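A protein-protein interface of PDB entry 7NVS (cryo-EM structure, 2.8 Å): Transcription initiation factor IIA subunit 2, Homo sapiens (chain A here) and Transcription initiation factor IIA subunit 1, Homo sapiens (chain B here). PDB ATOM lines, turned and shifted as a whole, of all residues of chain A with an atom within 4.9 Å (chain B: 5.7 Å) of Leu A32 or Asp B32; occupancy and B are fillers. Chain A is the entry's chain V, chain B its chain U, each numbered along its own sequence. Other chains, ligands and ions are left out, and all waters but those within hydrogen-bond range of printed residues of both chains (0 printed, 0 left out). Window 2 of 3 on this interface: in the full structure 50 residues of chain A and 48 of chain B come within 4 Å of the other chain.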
ATOM      1  N   ILE A  28     -22.489  -5.520  24.238  1.00  0.00           N
ATOM      2  CA  ILE A  28     -23.122  -4.297  24.720  1.00  0.00           C
ATOM      3  C   ILE A  28     -23.760  -4.575  26.074  1.00  0.00           C
ATOM      4  O   ILE A  28     -24.398  -5.615  26.272  1.00  0.00           O
ATOM      5  CB  ILE A  28     -24.169  -3.768  23.718  1.00  0.00           C
ATOM      6  CG1 ILE A  28     -25.328  -4.759  23.570  1.00  0.00           C
ATOM      7  CG2 ILE A  28     -23.517  -3.499  22.371  1.00  0.00           C
ATOM      8  CD1 ILE A  28     -26.376  -4.332  22.561  1.00  0.00           C
ATOM      9  N   THR A  29     -23.581  -3.644  27.006  1.00  0.00           N
ATOM     10  CA  THR A  29     -24.216  -3.748  28.308  1.00  0.00           C
ATOM     11  C   THR A  29     -25.706  -3.426  28.191  1.00  0.00           C
ATOM     12  O   THR A  29     -26.122  -2.712  27.274  1.00  0.00           O
ATOM     13  CB  THR A  29     -23.555  -2.794  29.300  1.00  0.00           C
ATOM     14  OG1 THR A  29     -24.019  -3.071  30.627  1.00  0.00           O
ATOM     15  CG2 THR A  29     -23.873  -1.346  28.949  1.00  0.00           C
ATOM     16  N   PRO A  30     -26.536  -3.944  29.103  1.00  0.00           N
ATOM     17  CA  PRO A  30     -27.976  -3.645  29.015  1.00  0.00           C
ATOM     18  C   PRO A  30     -28.286  -2.159  29.042  1.00  0.00           C
ATOM     19  O   PRO A  30     -29.258  -1.727  28.410  1.00  0.00           O
ATOM     20  CB  PRO A  30     -28.560  -4.369  30.235  1.00  0.00           C
ATOM     21  CG  PRO A  30     -27.592  -5.456  30.531  1.00  0.00           C
ATOM     22  CD  PRO A  30     -26.242  -4.913  30.173  1.00  0.00           C
ATOM     23  N   GLN A  31     -27.490  -1.361  29.758  1.00  0.00           N
ATOM     24  CA  GLN A  31     -27.727   0.078  29.789  1.00  0.00           C
ATOM     25  C   GLN A  31     -27.597   0.686  28.398  1.00  0.00           C
ATOM     26  O   GLN A  31     -28.388   1.558  28.017  1.00  0.00           O
ATOM     27  CB  GLN A  31     -26.753   0.748  30.760  1.00  0.00           C
ATOM     28  CG  GLN A  31     -26.990   2.239  30.943  1.00  0.00           C
ATOM     29  CD  GLN A  31     -26.081   2.847  31.993  1.00  0.00           C
ATOM     30  OE1 GLN A  31     -25.235   2.164  32.571  1.00  0.00           O
ATOM     31  NE2 GLN A  31     -26.252   4.139  32.247  1.00  0.00           N
ATOM     32  N   LEU A  32     -26.606   0.239  27.625  1.00  0.00           N
ATOM     33  CA  LEU A  32     -26.422   0.773  26.279  1.00  0.00           C
ATOM     34  C   LEU A  32     -27.629   0.474  25.401  1.00  0.00           C
ATOM     35  O   LEU A  32     -28.067   1.330  24.621  1.00  0.00           O
ATOM     36  CB  LEU A  32     -25.150   0.195  25.657  1.00  0.00           C
ATOM     37  CG  LEU A  32     -24.819   0.676  24.242  1.00  0.00           C
ATOM     38  CD1 LEU A  32     -24.761   2.193  24.190  1.00  0.00           C
ATOM     39  CD2 LEU A  32     -23.510   0.072  23.760  1.00  0.00           C
ATOM     40  N   ALA A  33     -28.182  -0.737  25.510  1.00  0.00           N
ATOM     41  CA  ALA A  33     -29.354  -1.084  24.713  1.00  0.00           C
ATOM     42  C   ALA A  33     -30.529  -0.172  25.037  1.00  0.00           C
ATOM     43  O   ALA A  33     -31.244   0.277  24.133  1.00  0.00           O
ATOM     44  CB  ALA A  33     -29.730  -2.547  24.947  1.00  0.00           C
ATOM     45  N   LEU A  34     -30.746   0.113  26.323  1.00  0.00           N
ATOM     46  CA  LEU A  34     -31.822   1.022  26.703  1.00  0.00           C
ATOM     47  C   LEU A  34     -31.591   2.414  26.128  1.00  0.00           C
ATOM     48  O   LEU A  34     -32.528   3.054  25.636  1.00  0.00           O
ATOM     49  CB  LEU A  34     -31.943   1.084  28.226  1.00  0.00           C
ATOM     50  CG  LEU A  34     -32.951   0.117  28.847  1.00  0.00           C
ATOM     51  CD1 LEU A  34     -32.440  -1.313  28.773  1.00  0.00           C
ATOM     52  CD2 LEU A  34     -33.253   0.508  30.286  1.00  0.00           C
ATOM     53  N   GLN A  35     -30.350   2.900  26.182  1.00  0.00           N
ATOM     54  CA  GLN A  35     -30.045   4.206  25.610  1.00  0.00           C
ATOM     55  C   GLN A  35     -30.290   4.217  24.106  1.00  0.00           C
ATOM     56  O   GLN A  35     -30.835   5.186  23.564  1.00  0.00           O
ATOM     57  CB  GLN A  35     -28.598   4.589  25.919  1.00  0.00           C
ATOM     58  CG  GLN A  35     -28.329   4.857  27.391  1.00  0.00           C
ATOM     59  CD  GLN A  35     -29.002   6.123  27.886  1.00  0.00           C
ATOM     60  OE1 GLN A  35     -28.604   7.232  27.531  1.00  0.00           O
ATOM     61  NE2 GLN A  35     -30.030   5.961  28.712  1.00  0.00           N
ATOM     62  N   VAL A  36     -29.896   3.146  23.414  1.00  0.00           N
ATOM     63  CA  VAL A  36     -30.119   3.071  21.973  1.00  0.00           C
ATOM     64  C   VAL A  36     -31.611   3.109  21.668  1.00  0.00           C
ATOM     65  O   VAL A  36     -32.054   3.801  20.742  1.00  0.00           O
ATOM     66  CB  VAL A  36     -29.455   1.808  21.396  1.00  0.00           C
ATOM     67  CG1 VAL A  36     -29.978   1.519  19.995  1.00  0.00           C
ATOM     68  CG2 VAL A  36     -27.942   1.964  21.384  1.00  0.00           C
ATOM     69  N   ASP B  27     -23.168  10.400  19.710  1.00  0.00           N
ATOM     70  CA  ASP B  27     -22.741  11.088  20.923  1.00  0.00           C
ATOM     71  C   ASP B  27     -22.866  10.182  22.143  1.00  0.00           C
ATOM     72  O   ASP B  27     -22.000  10.193  23.025  1.00  0.00           O
ATOM     73  CB  ASP B  27     -23.553  12.369  21.115  1.00  0.00           C
ATOM     74  CG  ASP B  27     -25.002  12.096  21.468  1.00  0.00           C
ATOM     75  OD1 ASP B  27     -25.814  11.900  20.540  1.00  0.00           O
ATOM     76  OD2 ASP B  27     -25.329  12.080  22.674  1.00  0.00           O
ATOM     77  N   ILE B  28     -23.939   9.390  22.210  1.00  0.00           N
ATOM     78  CA  ILE B  28     -24.123   8.487  23.342  1.00  0.00           C
ATOM     79  C   ILE B  28     -23.008   7.450  23.380  1.00  0.00           C
ATOM     80  O   ILE B  28     -22.452   7.152  24.444  1.00  0.00           O
ATOM     81  CB  ILE B  28     -25.510   7.820  23.274  1.00  0.00           C
ATOM     82  CG1 ILE B  28     -26.620   8.876  23.224  1.00  0.00           C
ATOM     83  CG2 ILE B  28     -25.711   6.890  24.463  1.00  0.00           C
ATOM     84  CD1 ILE B  28     -26.650   9.812  24.420  1.00  0.00           C
ATOM     85  N   PHE B  29     -22.662   6.884  22.222  1.00  0.00           N
ATOM     86  CA  PHE B  29     -21.603   5.881  22.177  1.00  0.00           C
ATOM     87  C   PHE B  29     -20.260   6.482  22.573  1.00  0.00           C
ATOM     88  O   PHE B  29     -19.459   5.831  23.254  1.00  0.00           O
ATOM     89  CB  PHE B  29     -21.527   5.260  20.780  1.00  0.00           C
ATOM     90  CG  PHE B  29     -22.766   4.500  20.376  1.00  0.00           C
ATOM     91  CD1 PHE B  29     -23.789   4.261  21.283  1.00  0.00           C
ATOM     92  CD2 PHE B  29     -22.904   4.023  19.084  1.00  0.00           C
ATOM     93  CE1 PHE B  29     -24.921   3.564  20.906  1.00  0.00           C
ATOM     94  CE2 PHE B  29     -24.036   3.324  18.705  1.00  0.00           C
ATOM     95  CZ  PHE B  29     -25.043   3.096  19.617  1.00  0.00           C
ATOM     96  N   LEU B  30     -19.986   7.714  22.142  1.00  0.00           N
ATOM     97  CA  LEU B  30     -18.768   8.386  22.580  1.00  0.00           C
ATOM     98  C   LEU B  30     -18.802   8.666  24.079  1.00  0.00           C
ATOM     99  O   LEU B  30     -17.785   8.525  24.766  1.00  0.00           O
ATOM    100  CB  LEU B  30     -18.574   9.686  21.798  1.00  0.00           C
ATOM    101  CG  LEU B  30     -17.733   9.575  20.524  1.00  0.00           C
ATOM    102  CD1 LEU B  30     -18.512   8.881  19.416  1.00  0.00           C
ATOM    103  CD2 LEU B  30     -17.267  10.951  20.072  1.00  0.00           C
ATOM    104  N   ASP B  31     -19.964   9.063  24.601  1.00  0.00           N
ATOM    105  CA  ASP B  31     -20.060   9.426  26.012  1.00  0.00           C
ATOM    106  C   ASP B  31     -19.851   8.216  26.914  1.00  0.00           C
ATOM    107  O   ASP B  31     -19.086   8.278  27.884  1.00  0.00           O
ATOM    108  CB  ASP B  31     -21.416  10.076  26.290  1.00  0.00           C
ATOM    109  CG  ASP B  31     -21.417  10.901  27.562  1.00  0.00           C
ATOM    110  OD1 ASP B  31     -20.681  10.546  28.506  1.00  0.00           O
ATOM    111  OD2 ASP B  31     -22.156  11.907  27.619  1.00  0.00           O
ATOM    112  N   ASP B  32     -20.522   7.102  26.612  1.00  0.00           N
ATOM    113  CA  ASP B  32     -20.444   5.928  27.476  1.00  0.00           C
ATOM    114  C   ASP B  32     -19.110   5.200  27.365  1.00  0.00           C
ATOM    115  O   ASP B  32     -18.857   4.289  28.160  1.00  0.00           O
ATOM    116  CB  ASP B  32     -21.597   4.968  27.164  1.00  0.00           C
ATOM    117  CG  ASP B  32     -21.348   4.128  25.927  1.00  0.00           C
ATOM    118  OD1 ASP B  32     -20.542   4.540  25.069  1.00  0.00           O
ATOM    119  OD2 ASP B  32     -21.965   3.048  25.811  1.00  0.00           O
ATOM    120  N   GLY B  33     -18.262   5.570  26.409  1.00  0.00           N
ATOM    121  CA  GLY B  33     -16.948   4.968  26.299  1.00  0.00           C
ATOM    122  C   GLY B  33     -16.901   3.658  25.549  1.00  0.00           C
ATOM    123  O   GLY B  33     -15.880   2.963  25.606  1.00  0.00           O
ATOM    124  N   VAL B  34     -17.968   3.294  24.845  1.00  0.00           N
ATOM    125  CA  VAL B  34     -18.015   2.064  24.060  1.00  0.00           C
ATOM    126  C   VAL B  34     -17.471   2.353  22.669  1.00  0.00           C
ATOM    127  O   VAL B  34     -17.710   3.429  22.104  1.00  0.00           O
ATOM    128  CB  VAL B  34     -19.448   1.502  23.992  1.00  0.00           C
ATOM    129  CG1 VAL B  34     -19.532   0.373  22.974  1.00  0.00           C
ATOM    130  CG2 VAL B  34     -19.887   1.018  25.366  1.00  0.00           C
ATOM    131  N   VAL B  38     -19.204  -0.977  17.531  1.00  0.00           N
ATOM    132  CA  VAL B  38     -20.456  -1.636  17.896  1.00  0.00           C
ATOM    133  C   VAL B  38     -21.576  -1.197  16.961  1.00  0.00           C
ATOM    134  O   VAL B  38     -22.406  -2.008  16.532  1.00  0.00           O
ATOM    135  CB  VAL B  38     -20.804  -1.344  19.367  1.00  0.00           C
ATOM    136  CG1 VAL B  38     -22.264  -1.671  19.647  1.00  0.00           C
ATOM    137  CG2 VAL B  38     -19.891  -2.131  20.294  1.00  0.00           C
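O of Phe B29 lies close to OD1 of Asp B32 (2.5 Å). O of Phe B29 sits at hydrogen-bond distance from N of Val B34 (3.3 Å). The side-chain carboxylate of Asp B32 lies within hydrogen-bond range of the backbone NH of Val B34 (2.9 Å).
Among the printed residues, pairs that only touch across the chains: Ile A28 with Val B38 (3.5 Å), Leu A32 with Phe B29 (3.6 Å), Leu A32 with Asp B32 (3.3 Å), Gln A35 with Ile B28 (3.97 Å) and Val A36 with Phe B29 (3.5 Å).
Of chain B, only Phe B29 (3.6 Å) and Asp B32 (3.3 Å) come within 4 Å of Leu A32. Asp B32 touches one residue of chain A. Of the printed residues of chain A, Phe B29 touches Leu A32 (3.6 Å) and Val A36 (3.5 Å). Of the printed residues of chain A, Ile B28 touches Gln A35 (3.97 Å). Of the printed residues of chain A, Val B38 touches Ile A28 (3.5 Å). Of the printed residues of chain B, Gln A35 touches Ile B28. Of the printed residues of chain B, Val A36 touches Phe B29 (3.5 Å). Gln A31 touches none of the printed residues of chain B. Gly B33 touches none of the printed residues of chain A. The nearest printed residue of chain A that does not touch Asp B32 is Thr A29 (5.7 Å). The nearest printed residue of chain A that does not touch Val B38 is Leu A32 (4.6 Å).
Hydrophobic or aromatic side chains of chain B that line the printed part of chain A: Ile B28, Phe B29 and Val B38. Hydrophobic or aromatic side chains of chain A that line the printed part of chain B: Ile A28, Leu A32 and Val A36. Along chain A the printed residues that touch a printed residue of chain B span positions 28 to 36. Among the printed residues, no Asp or Glu carboxylate lies within 4 Å of a Lys or Arg side-chain nitrogen of the other chain.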
